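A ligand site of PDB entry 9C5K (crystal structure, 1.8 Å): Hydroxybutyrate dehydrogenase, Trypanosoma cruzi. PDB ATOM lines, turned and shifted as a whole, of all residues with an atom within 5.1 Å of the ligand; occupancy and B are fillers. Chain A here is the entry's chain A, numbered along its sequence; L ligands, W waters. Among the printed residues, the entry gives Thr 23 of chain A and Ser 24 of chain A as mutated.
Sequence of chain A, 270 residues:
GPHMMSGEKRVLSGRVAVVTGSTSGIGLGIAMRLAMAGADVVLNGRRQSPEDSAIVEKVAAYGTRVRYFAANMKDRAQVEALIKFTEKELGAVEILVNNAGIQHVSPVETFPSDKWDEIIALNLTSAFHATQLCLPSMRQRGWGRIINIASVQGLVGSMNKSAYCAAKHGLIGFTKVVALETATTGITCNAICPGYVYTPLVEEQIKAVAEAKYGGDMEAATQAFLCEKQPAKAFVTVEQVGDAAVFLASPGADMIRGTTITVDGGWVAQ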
ATOM      1  N   GLY A  21       8.306  22.186  18.396  1.00  0.00           N
ATOM      2  CA  GLY A  21       6.937  21.956  17.936  1.00  0.00           C
ATOM      3  C   GLY A  21       6.631  22.534  16.572  1.00  0.00           C
ATOM      4  O   GLY A  21       5.683  23.310  16.405  1.00  0.00           O
ATOM      5  N   SER A  22       7.410  22.138  15.568  1.00  0.00           N
ATOM      6  CA  SER A  22       7.352  22.759  14.251  1.00  0.00           C
ATOM      7  C   SER A  22       6.919  21.769  13.176  1.00  0.00           C
ATOM      8  O   SER A  22       7.252  21.927  12.000  1.00  0.00           O
ATOM      9  CB  SER A  22       8.702  23.413  13.918  1.00  0.00           C
ATOM     10  OG  SER A  22       9.766  22.544  14.260  1.00  0.00           O
ATOM     11  N   THR A  23       6.139  20.755  13.554  1.00  0.00           N
ATOM     12  CA  THR A  23       5.548  19.788  12.633  1.00  0.00           C
ATOM     13  C   THR A  23       4.168  20.206  12.130  1.00  0.00           C
ATOM     14  O   THR A  23       3.569  19.490  11.317  1.00  0.00           O
ATOM     15  CB  THR A  23       5.414  18.432  13.315  1.00  0.00           C
ATOM     16  OG1 THR A  23       4.437  18.544  14.374  1.00  0.00           O
ATOM     17  CG2 THR A  23       6.734  18.000  13.905  1.00  0.00           C
ATOM     18  N   SER A  24       3.643  21.326  12.618  1.00  0.00           N
ATOM     19  CA  SER A  24       2.243  21.696  12.497  1.00  0.00           C
ATOM     20  C   SER A  24       2.138  23.195  12.799  1.00  0.00           C
ATOM     21  O   SER A  24       3.004  23.779  13.476  1.00  0.00           O
ATOM     22  CB  SER A  24       1.376  20.879  13.484  1.00  0.00           C
ATOM     23  OG  SER A  24       0.014  21.304  13.526  1.00  0.00           O
ATOM     24  N   GLY A  25       1.073  23.804  12.286  1.00  0.00           N
ATOM     25  CA  GLY A  25       0.615  25.078  12.821  1.00  0.00           C
ATOM     26  C   GLY A  25       1.639  26.193  12.726  1.00  0.00           C
ATOM     27  O   GLY A  25       2.344  26.372  11.712  1.00  0.00           O
ATOM     28  N   ILE A  26       1.666  26.998  13.790  1.00  0.00           N
ATOM     29  CA  ILE A  26       2.518  28.189  13.854  1.00  0.00           C
ATOM     30  C   ILE A  26       3.991  27.815  13.768  1.00  0.00           C
ATOM     31  O   ILE A  26       4.792  28.467  13.070  1.00  0.00           O
ATOM     32  CB  ILE A  26       2.203  28.980  15.141  1.00  0.00           C
ATOM     33  CG1 ILE A  26       0.821  29.617  15.025  1.00  0.00           C
ATOM     34  CG2 ILE A  26       3.276  30.007  15.460  1.00  0.00           C
ATOM     35  CD1 ILE A  26       0.260  30.146  16.376  1.00  0.00           C
ATOM     36  N   GLY A  27       4.382  26.751  14.492  1.00  0.00           N
ATOM     37  CA  GLY A  27       5.792  26.383  14.512  1.00  0.00           C
ATOM     38  C   GLY A  27       6.297  26.108  13.106  1.00  0.00           C
ATOM     39  O   GLY A  27       7.398  26.561  12.712  1.00  0.00           O
ATOM     40  N   ASN A  44      11.073  20.057  14.993  1.00  0.00           N
ATOM     41  CA  ASN A  44      10.920  19.229  16.172  1.00  0.00           C
ATOM     42  C   ASN A  44       9.460  18.927  16.463  1.00  0.00           C
ATOM     43  O   ASN A  44       8.578  19.756  16.243  1.00  0.00           O
ATOM     44  CB  ASN A  44      11.548  19.921  17.391  1.00  0.00           C
ATOM     45  CG  ASN A  44      11.019  19.397  18.704  1.00  0.00           C
ATOM     46  OD1 ASN A  44      10.189  20.032  19.332  1.00  0.00           O
ATOM     47  ND2 ASN A  44      11.522  18.233  19.133  1.00  0.00           N
ATOM     48  N   GLY A  45       9.241  17.733  17.026  1.00  0.00           N
ATOM     49  CA  GLY A  45       7.952  17.262  17.509  1.00  0.00           C
ATOM     50  C   GLY A  45       8.182  15.987  18.281  1.00  0.00           C
ATOM     51  O   GLY A  45       9.327  15.557  18.482  1.00  0.00           O
ATOM     52  N   ARG A  46       7.085  15.399  18.771  1.00  0.00           N
ATOM     53  CA  ARG A  46       7.228  14.230  19.644  1.00  0.00           C
ATOM     54  C   ARG A  46       7.518  12.933  18.890  1.00  0.00           C
ATOM     55  O   ARG A  46       8.048  11.986  19.489  1.00  0.00           O
ATOM     56  CB  ARG A  46       5.949  14.047  20.475  1.00  0.00           C
ATOM     57  CG  ARG A  46       5.734  15.128  21.523  1.00  0.00           C
ATOM     58  CD  ARG A  46       4.308  15.145  22.033  1.00  0.00           C
ATOM     59  NE  ARG A  46       3.383  15.587  20.990  1.00  0.00           N
ATOM     60  CZ  ARG A  46       2.063  15.630  21.134  1.00  0.00           C
ATOM     61  NH1 ARG A  46       1.477  15.227  22.254  1.00  0.00           N
ATOM     62  NH2 ARG A  46       1.330  16.094  20.142  1.00  0.00           N
ATOM     63  N   ARG A  47       7.126  12.851  17.617  1.00  0.00           N
ATOM     64  CA  ARG A  47       7.050  11.578  16.910  1.00  0.00           C
ATOM     65  C   ARG A  47       8.313  11.305  16.106  1.00  0.00           C
ATOM     66  O   ARG A  47       8.915  12.215  15.539  1.00  0.00           O
ATOM     67  CB  ARG A  47       5.848  11.558  15.948  1.00  0.00           C
ATOM     68  CG  ARG A  47       4.531  11.737  16.657  1.00  0.00           C
ATOM     69  CD  ARG A  47       3.295  11.581  15.767  1.00  0.00           C
ATOM     70  NE  ARG A  47       2.388  12.700  16.009  1.00  0.00           N
ATOM     71  CZ  ARG A  47       1.868  13.030  17.194  1.00  0.00           C
ATOM     72  NH1 ARG A  47       2.036  12.256  18.268  1.00  0.00           N
ATOM     73  NH2 ARG A  47       1.177  14.158  17.311  1.00  0.00           N
ATOM     74  N   PRO A  50       6.576  12.362  12.049  1.00  0.00           N
ATOM     75  CA  PRO A  50       5.465  13.317  12.172  1.00  0.00           C
ATOM     76  C   PRO A  50       4.323  12.962  11.216  1.00  0.00           C
ATOM     77  O   PRO A  50       4.493  12.287  10.203  1.00  0.00           O
ATOM     78  CB  PRO A  50       6.103  14.662  11.788  1.00  0.00           C
ATOM     79  CG  PRO A  50       7.574  14.455  11.855  1.00  0.00           C
ATOM     80  CD  PRO A  50       7.796  13.009  11.518  1.00  0.00           C
ATOM     81  N   ALA A  71      11.788  14.999  19.909  1.00  0.00           N
ATOM     82  CA  ALA A  71      12.085  15.157  21.333  1.00  0.00           C
ATOM     83  C   ALA A  71      10.867  15.744  22.018  1.00  0.00           C
ATOM     84  O   ALA A  71      10.327  16.739  21.542  1.00  0.00           O
ATOM     85  CB  ALA A  71      13.266  16.089  21.512  1.00  0.00           C
ATOM     86  N   ASN A  72      10.499  15.163  23.162  1.00  0.00           N
ATOM     87  CA  ASN A  72       9.406  15.700  23.969  1.00  0.00           C
ATOM     88  C   ASN A  72       9.933  16.804  24.862  1.00  0.00           C
ATOM     89  O   ASN A  72      10.745  16.545  25.760  1.00  0.00           O
ATOM     90  CB  ASN A  72       8.754  14.594  24.789  1.00  0.00           C
ATOM     91  CG  ASN A  72       7.460  15.035  25.406  1.00  0.00           C
ATOM     92  OD1 ASN A  72       7.376  16.117  25.976  1.00  0.00           O
ATOM     93  ND2 ASN A  72       6.415  14.215  25.247  1.00  0.00           N
ATOM     94  N   MET A  73       9.470  18.032  24.629  1.00  0.00           N
ATOM     95  CA  MET A  73      10.008  19.197  25.319  1.00  0.00           C
ATOM     96  C   MET A  73       9.671  19.229  26.808  1.00  0.00           C
ATOM     97  O   MET A  73      10.243  20.055  27.544  1.00  0.00           O
ATOM     98  CB  MET A  73       9.504  20.480  24.605  1.00  0.00           C
ATOM     99  CG  MET A  73      10.048  20.651  23.187  1.00  0.00           C
ATOM    100  SD  MET A  73      11.839  20.879  23.169  1.00  0.00           S
ATOM    101  CE  MET A  73      12.455  19.259  22.718  1.00  0.00           C
ATOM    102  N   LYS A  74       8.767  18.371  27.282  1.00  0.00           N
ATOM    103  CA  LYS A  74       8.501  18.300  28.715  1.00  0.00           C
ATOM    104  C   LYS A  74       9.566  17.537  29.489  1.00  0.00           C
ATOM    105  O   LYS A  74       9.457  17.428  30.712  1.00  0.00           O
ATOM    106  CB  LYS A  74       7.129  17.654  28.975  1.00  0.00           C
ATOM    107  CG  LYS A  74       5.947  18.484  28.450  1.00  0.00           C
ATOM    108  CD  LYS A  74       4.600  17.821  28.701  1.00  0.00           C
ATOM    109  CE  LYS A  74       4.473  16.617  27.825  1.00  0.00           C
ATOM    110  NZ  LYS A  74       3.161  15.893  28.063  1.00  0.00           N
ATOM    111  N   ASN A  99       8.211  27.306  20.872  1.00  0.00           N
ATOM    112  CA  ASN A  99       6.859  27.349  20.309  1.00  0.00           C
ATOM    113  C   ASN A  99       5.966  26.204  20.731  1.00  0.00           C
ATOM    114  O   ASN A  99       4.739  26.382  20.794  1.00  0.00           O
ATOM    115  CB  ASN A  99       6.965  27.382  18.765  1.00  0.00           C
ATOM    116  CG  ASN A  99       5.632  27.147  18.073  1.00  0.00           C
ATOM    117  OD1 ASN A  99       4.862  28.089  17.826  1.00  0.00           O
ATOM    118  ND2 ASN A  99       5.390  25.907  17.712  1.00  0.00           N
ATOM    119  N   ALA A 100       6.494  25.014  20.987  1.00  0.00           N
ATOM    120  CA  ALA A 100       5.591  23.902  21.262  1.00  0.00           C
ATOM    121  C   ALA A 100       4.688  24.199  22.448  1.00  0.00           C
ATOM    122  O   ALA A 100       5.144  24.713  23.474  1.00  0.00           O
ATOM    123  CB  ALA A 100       6.379  22.627  21.525  1.00  0.00           C
ATOM    124  N   GLY A 101       3.422  23.821  22.319  1.00  0.00           N
ATOM    125  CA  GLY A 101       2.445  24.223  23.314  1.00  0.00           C
ATOM    126  C   GLY A 101       1.143  23.483  23.123  1.00  0.00           C
ATOM    127  O   GLY A 101       0.821  23.030  22.015  1.00  0.00           O
ATOM    128  N   ILE A 102       0.396  23.370  24.224  1.00  0.00           N
ATOM    129  CA  ILE A 102      -0.877  22.654  24.247  1.00  0.00           C
ATOM    130  C   ILE A 102      -1.921  23.516  24.953  1.00  0.00           C
ATOM    131  O   ILE A 102      -1.603  24.465  25.655  1.00  0.00           O
ATOM    132  CB  ILE A 102      -0.807  21.284  24.936  1.00  0.00           C
ATOM    133  CG1 ILE A 102      -0.229  21.405  26.354  1.00  0.00           C
ATOM    134  CG2 ILE A 102       0.039  20.357  24.101  1.00  0.00           C
ATOM    135  CD1 ILE A 102      -0.267  20.098  27.146  1.00  0.00           C
ATOM    136  N   LEU A 122       4.939  22.295  29.660  1.00  0.00           N
ATOM    137  CA  LEU A 122       5.291  22.524  28.262  1.00  0.00           C
ATOM    138  C   LEU A 122       5.261  23.994  27.925  1.00  0.00           C
ATOM    139  O   LEU A 122       6.178  24.489  27.255  1.00  0.00           O
ATOM    140  CB  LEU A 122       4.341  21.770  27.328  1.00  0.00           C
ATOM    141  CG  LEU A 122       4.684  21.902  25.845  1.00  0.00           C
ATOM    142  CD1 LEU A 122       6.080  21.337  25.504  1.00  0.00           C
ATOM    143  CD2 LEU A 122       3.600  21.209  25.040  1.00  0.00           C
ATOM    144  N   ASN A 123       4.234  24.718  28.317  1.00  0.00           N
ATOM    145  CA  ASN A 123       4.078  26.074  27.800  1.00  0.00           C
ATOM    146  C   ASN A 123       4.950  27.103  28.542  1.00  0.00           C
ATOM    147  O   ASN A 123       5.049  28.266  28.093  1.00  0.00           O
ATOM    148  CB  ASN A 123       2.629  26.523  27.886  1.00  0.00           C
ATOM    149  CG  ASN A 123       1.666  25.712  26.988  1.00  0.00           C
ATOM    150  OD1 ASN A 123       1.975  24.602  26.453  1.00  0.00           O
ATOM    151  ND2 ASN A 123       0.460  26.231  26.878  1.00  0.00           N
ATOM    152  N   ILE A 149       7.002  32.015  21.822  1.00  0.00           N
ATOM    153  CA  ILE A 149       5.659  32.167  21.281  1.00  0.00           C
ATOM    154  C   ILE A 149       4.713  32.109  22.467  1.00  0.00           C
ATOM    155  O   ILE A 149       4.402  31.053  23.007  1.00  0.00           O
ATOM    156  CB  ILE A 149       5.349  31.106  20.228  1.00  0.00           C
ATOM    157  CG1 ILE A 149       6.462  31.071  19.165  1.00  0.00           C
ATOM    158  CG2 ILE A 149       3.975  31.382  19.586  1.00  0.00           C
ATOM    159  CD1 ILE A 149       6.742  32.462  18.461  1.00  0.00           C
ATOM    160  N   ALA A 150       4.230  33.269  22.860  1.00  0.00           N
ATOM    161  CA  ALA A 150       3.292  33.462  23.943  1.00  0.00           C
ATOM    162  C   ALA A 150       1.929  33.472  23.290  1.00  0.00           C
ATOM    163  O   ALA A 150       1.568  32.465  22.702  1.00  0.00           O
ATOM    164  CB  ALA A 150       3.598  34.712  24.752  1.00  0.00           C
ATOM    165  N   SER A 151       1.090  34.445  23.633  1.00  0.00           N
ATOM    166  CA  SER A 151      -0.290  34.514  23.221  1.00  0.00           C
ATOM    167  C   SER A 151      -0.819  35.838  23.734  1.00  0.00           C
ATOM    168  O   SER A 151      -0.297  36.392  24.710  1.00  0.00           O
ATOM    169  CB  SER A 151      -1.080  33.358  23.825  1.00  0.00           C
ATOM    170  OG  SER A 151      -2.467  33.553  23.630  1.00  0.00           O
ATOM    171  N   VAL A 152      -1.936  36.284  23.144  1.00  0.00           N
ATOM    172  CA  VAL A 152      -2.740  37.325  23.779  1.00  0.00           C
ATOM    173  C   VAL A 152      -3.151  36.849  25.166  1.00  0.00           C
ATOM    174  O   VAL A 152      -3.312  37.656  26.074  1.00  0.00           O
ATOM    175  CB  VAL A 152      -3.932  37.695  22.898  1.00  0.00           C
ATOM    176  CG1 VAL A 152      -4.858  38.639  23.643  1.00  0.00           C
ATOM    177  CG2 VAL A 152      -3.388  38.339  21.647  1.00  0.00           C
ATOM    178  N   TYR A 164      -3.552  27.749  30.862  1.00  0.00           N
ATOM    179  CA  TYR A 164      -2.912  28.328  29.683  1.00  0.00           C
ATOM    180  C   TYR A 164      -2.605  29.807  29.841  1.00  0.00           C
ATOM    181  O   TYR A 164      -1.495  30.254  29.527  1.00  0.00           O
ATOM    182  CB  TYR A 164      -3.809  28.078  28.497  1.00  0.00           C
ATOM    183  CG  TYR A 164      -3.290  28.456  27.138  1.00  0.00           C
ATOM    184  CD1 TYR A 164      -3.506  29.719  26.635  1.00  0.00           C
ATOM    185  CD2 TYR A 164      -2.712  27.506  26.332  1.00  0.00           C
ATOM    186  CE1 TYR A 164      -3.130  30.052  25.288  1.00  0.00           C
ATOM    187  CE2 TYR A 164      -2.306  27.817  25.033  1.00  0.00           C
ATOM    188  CZ  TYR A 164      -2.522  29.080  24.530  1.00  0.00           C
ATOM    189  OH  TYR A 164      -2.170  29.344  23.229  1.00  0.00           O
ATOM    190  N   LYS A 168       1.225  31.247  29.857  1.00  0.00           N
ATOM    191  CA  LYS A 168       1.592  32.261  28.871  1.00  0.00           C
ATOM    192  C   LYS A 168       1.961  33.594  29.524  1.00  0.00           C
ATOM    193  O   LYS A 168       2.899  34.252  29.067  1.00  0.00           O
ATOM    194  CB  LYS A 168       0.486  32.447  27.876  1.00  0.00           C
ATOM    195  CG  LYS A 168       0.246  31.233  27.031  1.00  0.00           C
ATOM    196  CD  LYS A 168       1.434  30.929  26.124  1.00  0.00           C
ATOM    197  CE  LYS A 168       1.010  29.938  25.021  1.00  0.00           C
ATOM    198  NZ  LYS A 168       2.164  29.560  24.143  1.00  0.00           N
ATOM    199  N   PRO A 194       0.450  36.031  19.400  1.00  0.00           N
ATOM    200  CA  PRO A 194      -0.613  35.940  18.380  1.00  0.00           C
ATOM    201  C   PRO A 194      -1.984  35.966  19.022  1.00  0.00           C
ATOM    202  O   PRO A 194      -2.154  35.441  20.131  1.00  0.00           O
ATOM    203  CB  PRO A 194      -0.356  34.589  17.697  1.00  0.00           C
ATOM    204  CG  PRO A 194       1.078  34.164  18.196  1.00  0.00           C
ATOM    205  CD  PRO A 194       1.160  34.758  19.576  1.00  0.00           C
ATOM    206  N   GLY A 195      -2.951  36.550  18.305  1.00  0.00           N
ATOM    207  CA  GLY A 195      -4.369  36.272  18.518  1.00  0.00           C
ATOM    208  C   GLY A 195      -4.688  34.938  17.885  1.00  0.00           C
ATOM    209  O   GLY A 195      -3.797  34.114  17.622  1.00  0.00           O
ATOM    210  N   TYR A 196      -5.975  34.694  17.656  1.00  0.00           N
ATOM    211  CA  TYR A 196      -6.324  33.396  17.124  1.00  0.00           C
ATOM    212  C   TYR A 196      -5.769  33.161  15.725  1.00  0.00           C
ATOM    213  O   TYR A 196      -5.914  34.001  14.832  1.00  0.00           O
ATOM    214  CB  TYR A 196      -7.826  33.229  17.066  1.00  0.00           C
ATOM    215  CG  TYR A 196      -8.569  33.094  18.374  1.00  0.00           C
ATOM    216  CD1 TYR A 196      -8.032  32.388  19.491  1.00  0.00           C
ATOM    217  CD2 TYR A 196      -9.842  33.633  18.498  1.00  0.00           C
ATOM    218  CE1 TYR A 196      -8.791  32.239  20.669  1.00  0.00           C
ATOM    219  CE2 TYR A 196     -10.589  33.478  19.683  1.00  0.00           C
ATOM    220  CZ  TYR A 196     -10.086  32.768  20.737  1.00  0.00           C
ATOM    221  OH  TYR A 196     -10.869  32.619  21.869  1.00  0.00           O
ATOM    222  N   VAL A 197      -5.251  31.940  15.532  1.00  0.00           N
ATOM    223  CA  VAL A 197      -4.683  31.438  14.277  1.00  0.00           C
ATOM    224  C   VAL A 197      -5.347  30.073  14.015  1.00  0.00           C
ATOM    225  O   VAL A 197      -5.580  29.312  14.969  1.00  0.00           O
ATOM    226  CB  VAL A 197      -3.153  31.269  14.418  1.00  0.00           C
ATOM    227  CG1 VAL A 197      -2.540  30.694  13.111  1.00  0.00           C
ATOM    228  CG2 VAL A 197      -2.515  32.558  14.753  1.00  0.00           C
ATOM    229  N   THR A 199      -5.262  26.752  13.506  1.00  0.00           N
ATOM    230  CA  THR A 199      -4.452  25.548  13.629  1.00  0.00           C
ATOM    231  C   THR A 199      -5.261  24.444  14.288  1.00  0.00           C
ATOM    232  O   THR A 199      -6.309  24.732  14.858  1.00  0.00           O
ATOM    233  CB  THR A 199      -3.245  25.799  14.519  1.00  0.00           C
ATOM    234  OG1 THR A 199      -3.740  26.044  15.846  1.00  0.00           O
ATOM    235  CG2 THR A 199      -2.442  27.030  14.075  1.00  0.00           C
ATOM    236  N   PRO A 200      -4.769  23.207  14.352  1.00  0.00           N
ATOM    237  CA  PRO A 200      -5.521  22.177  15.088  1.00  0.00           C
ATOM    238  C   PRO A 200      -5.821  22.555  16.525  1.00  0.00           C
ATOM    239  O   PRO A 200      -6.871  22.154  17.076  1.00  0.00           O
ATOM    240  CB  PRO A 200      -4.612  20.952  14.994  1.00  0.00           C
ATOM    241  CG  PRO A 200      -3.909  21.150  13.655  1.00  0.00           C
ATOM    242  CD  PRO A 200      -3.639  22.623  13.609  1.00  0.00           C
ATOM    243  N   LEU A 201      -4.940  23.316  17.175  1.00  0.00           N
ATOM    244  CA  LEU A 201      -5.199  23.700  18.551  1.00  0.00           C
ATOM    245  C   LEU A 201      -6.487  24.520  18.660  1.00  0.00           C
ATOM    246  O   LEU A 201      -7.225  24.387  19.632  1.00  0.00           O
ATOM    247  CB  LEU A 201      -4.011  24.494  19.076  1.00  0.00           C
ATOM    248  CG  LEU A 201      -4.059  24.882  20.545  1.00  0.00           C
ATOM    249  CD1 LEU A 201      -2.634  24.937  21.132  1.00  0.00           C
ATOM    250  CD2 LEU A 201      -4.656  26.271  20.614  1.00  0.00           C
ATOM    251  N   VAL A 202      -6.747  25.381  17.696  1.00  0.00           N
ATOM    252  CA  VAL A 202      -7.985  26.160  17.682  1.00  0.00           C
ATOM    253  C   VAL A 202      -9.127  25.373  17.045  1.00  0.00           C
ATOM    254  O   VAL A 202     -10.273  25.425  17.515  1.00  0.00           O
ATOM    255  CB  VAL A 202      -7.723  27.501  16.955  1.00  0.00           C
ATOM    256  CG1 VAL A 202      -8.998  28.084  16.402  1.00  0.00           C
ATOM    257  CG2 VAL A 202      -7.044  28.518  17.941  1.00  0.00           C
HETATM  258  P1  LIG L   1      -0.531  22.983  16.962  1.00  0.00           P
HETATM  259  O1  LIG L   1      -1.301  21.987  17.793  1.00  0.00           O
HETATM  260  O2  LIG L   1      -1.012  23.169  15.553  1.00  0.00           O
HETATM  261  O3  LIG L   1       1.043  22.624  16.970  1.00  0.00           O
HETATM  262  C1  LIG L   1       1.488  22.191  18.260  1.00  0.00           C
HETATM  263  C2  LIG L   1       2.947  21.723  17.972  1.00  0.00           C
HETATM  264  O4  LIG L   1       3.659  21.315  19.138  1.00  0.00           O
HETATM  265  C3  LIG L   1       2.879  20.541  16.960  1.00  0.00           C
HETATM  266  O5  LIG L   1       3.944  20.650  16.048  1.00  0.00           O
HETATM  267  C4  LIG L   1       3.203  19.261  17.835  1.00  0.00           C
HETATM  268  O6  LIG L   1       3.968  18.430  17.171  1.00  0.00           O
HETATM  269  C5  LIG L   1       4.152  19.940  18.947  1.00  0.00           C
HETATM  270  N1  LIG L   1       4.153  19.390  20.263  1.00  0.00           N
HETATM  271  C6  LIG L   1       3.095  19.177  21.119  1.00  0.00           C
HETATM  272  N2  LIG L   1       3.461  18.716  22.343  1.00  0.00           N
HETATM  273  C7  LIG L   1       4.845  18.631  22.223  1.00  0.00           C
HETATM  274  C8  LIG L   1       5.848  18.232  23.101  1.00  0.00           C
HETATM  275  N3  LIG L   1       5.534  17.779  24.378  1.00  0.00           N
HETATM  276  N4  LIG L   1       7.157  18.260  22.740  1.00  0.00           N
HETATM  277  C9  LIG L   1       7.403  18.709  21.456  1.00  0.00           C
HETATM  278  N5  LIG L   1       6.569  19.104  20.517  1.00  0.00           N
HETATM  279  C10 LIG L   1       5.276  19.092  20.936  1.00  0.00           C
HETATM  280  O7  LIG L   1      -0.951  24.365  17.800  1.00  0.00           O
HETATM  281  P2  LIG L   1      -0.421  25.835  17.322  1.00  0.00           P
HETATM  282  O8  LIG L   1       0.530  25.837  16.174  1.00  0.00           O
HETATM  283  O9  LIG L   1      -1.663  26.683  17.420  1.00  0.00           O
HETATM  284  O10 LIG L   1       0.465  26.207  18.656  1.00  0.00           O
HETATM  285  C11 LIG L   1       1.840  26.594  18.519  1.00  0.00           C
HETATM  286  C12 LIG L   1       2.090  27.644  19.645  1.00  0.00           C
HETATM  287  O11 LIG L   1       1.258  28.789  19.314  1.00  0.00           O
HETATM  288  C13 LIG L   1       1.577  27.170  21.053  1.00  0.00           C
HETATM  289  O12 LIG L   1       2.544  27.590  22.077  1.00  0.00           O
HETATM  290  C14 LIG L   1       0.314  27.917  21.240  1.00  0.00           C
HETATM  291  O13 LIG L   1       0.122  28.203  22.596  1.00  0.00           O
HETATM  292  C15 LIG L   1       0.699  29.253  20.457  1.00  0.00           C
HETATM  293  N6  LIG L   1      -0.439  30.054  20.141  1.00  0.00           N
HETATM  294  C16 LIG L   1      -1.528  29.561  19.315  1.00  0.00           C
HETATM  295  C17 LIG L   1      -2.536  30.400  18.962  1.00  0.00           C
HETATM  296  C18 LIG L   1      -3.636  29.937  18.062  1.00  0.00           C
HETATM  297  O14 LIG L   1      -4.633  30.582  17.879  1.00  0.00           O
HETATM  298  N7  LIG L   1      -3.476  28.784  17.363  1.00  0.00           N
HETATM  299  C19 LIG L   1      -2.614  31.772  19.358  1.00  0.00           C
HETATM  300  C20 LIG L   1      -1.489  32.186  20.211  1.00  0.00           C
HETATM  301  C21 LIG L   1      -0.487  31.382  20.558  1.00  0.00           C
HETATM  302  P3  LIG L   1       3.716  16.691  17.310  1.00  0.00           P
HETATM  303  O15 LIG L   1       4.249  16.381  15.933  1.00  0.00           O
HETATM  304  O16 LIG L   1       4.589  16.271  18.494  1.00  0.00           O
HETATM  305  O17 LIG L   1       2.231  16.613  17.489  1.00  0.00           O
HETATM  306  O   HOH W   1       2.965  24.867  16.134  1.00  0.00           O
HETATM  307  O   HOH W   2       6.258  14.622  15.539  1.00  0.00           O
HETATM  308  O   HOH W   3       2.520  17.501  24.774  1.00  0.00           O
HETATM  309  O   HOH W   4      -0.093  19.085  20.228  1.00  0.00           O
HETATM  310  O   HOH W   5      -1.111  21.636  20.820  1.00  0.00           O
HETATM  311  O   HOH W   6       2.776  15.346  13.978  1.00  0.00           O
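ND2 of Asn 99 sits close to N of Gly 27. The backbone carbonyl oxygen (O) of Ala 150 is in hydrogen-bond range of the side-chain amino group (NZ) of Lys 168 (3.3 Å). N of Val 152 sits at hydrogen-bond distance from O of Pro 194. The backbone NH (N) of Gly 21 lies within hydrogen-bond range of the side-chain amide oxygen (OD1) of Asn 44 (3.0 Å). N of Leu 201 lies close to OG1 of Thr 199, at 3.3 Å. NZ of Lys 168 lies within hydrogen-bond range of O of Ile 149 (2.9 Å). The backbone NH (N) of Ala 71 sits at hydrogen-bond distance from the backbone carbonyl oxygen (O) of Gly 45, 2.9 Å away. ND2 of Asn 99 is in hydrogen-bond range of O of Gly 21, at 2.9 Å.
Water W6 bridges an oxygen (O15) of the ligand and the guanidinium group of Arg 47. Water W2 lies within hydrogen-bond range of an oxygen (O15) of the ligand (2.7 Å), the backbone NH (N) of Arg 47 (2.9 Å) and the backbone NH (N) of Arg 46 (3.4 Å). Water W5 lies within hydrogen-bond range of the backbone carbonyl oxygen of Gly 101 (2.7 Å) and an oxygen (O1) of the ligand (3.1 Å).
Merely in contact with the ligand: Gly 195 (3.1 Å), Ala 150 (3.2 Å), Val 202 (3.2 Å), Pro 200 (3.3 Å), Leu 201 (3.3 Å), Pro 194 (3.3 Å), Tyr 196 (3.4 Å), Gly 25 (3.4 Å), Ala 71 (3.5 Å), Gly 101 (3.6 Å), Gly 45 (3.6 Å), Ala 100 (3.7 Å), Leu 122 (3.7 Å), Asn 44 (3.7 Å), Ile 149 (3.8 Å), Lys 74 (3.8 Å), Ser 22 (3.8 Å) and Ser 151 (3.8 Å). Hydrophobic or aromatic side chains that line the ligand: Ile 26, Met 73, Ala 100, Leu 122, Ile 149, Tyr 164, Pro 194, Val 197, Pro 200, Leu 201 and Val 202. 31 residues have an atom within 4 Å of the ligand: Gly 21, Ser 22, Thr 23, Ser 24, Gly 25, Ile 26, Asn 44, Gly 45, Arg 46, Arg 47, Ala 71, Asn 72, Met 73, Lys 74, Asn 99, Ala 100, Gly 101, Leu 122, Ile 149, Ala 150, Ser 151, Tyr 164, Lys 168, Pro 194, Gly 195, Tyr 196, Val 197, Thr 199, Pro 200, Leu 201 and Val 202.
The guanidinium group (NH2) of Arg 47 is in salt-bridge range of an oxygen (O17) of the ligand (2.7 Å). The backbone carbonyl oxygen (O) of Gly 21 sits at hydrogen-bond distance from an oxygen (O5) of the ligand (3.2 Å). OG of Ser 24 sits at hydrogen-bond distance from O2 of the ligand, at 2.9 Å. NZ of Lys 168 lies within hydrogen-bond range of O12 of the ligand. O of Val 197 is in hydrogen-bond range of N7 of the ligand, 3.2 Å away. OD1 of Asn 72 lies within hydrogen-bond range of N3 of the ligand, 3.0 Å away. An oxygen (O17) of the ligand is in salt-bridge range of the guanidinium group (NH2) of Arg 46 (2.8 Å). O16 of the ligand sits at hydrogen-bond distance from N of Arg 46, at 2.7 Å. The backbone NH (N) of Met 73 lies within hydrogen-bond range of a nitrogen (N4) of the ligand (3.0 Å). The side-chain hydroxyl (OG1) of Thr 199 lies within hydrogen-bond range of an oxygen (O9) of the ligand. The backbone carbonyl oxygen (O) of Asn 99 sits at hydrogen-bond distance from an oxygen (O12) of the ligand, at 2.8 Å. N of Ile 26 lies within hydrogen-bond range of O8 of the ligand, at 2.9 Å. The backbone NH of Thr 23 lies within hydrogen-bond range of an oxygen (O5) of the ligand (3.3 Å). An oxygen (O13) of the ligand lies within hydrogen-bond range of the side-chain hydroxyl of Tyr 164, at 2.6 Å. The backbone NH (N) of Val 197 is in hydrogen-bond range of an oxygen (O14) of the ligand (2.8 Å). The side-chain hydroxyl of Thr 23 lies within hydrogen-bond range of an oxygen (O15) of the ligand, 2.7 Å away.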
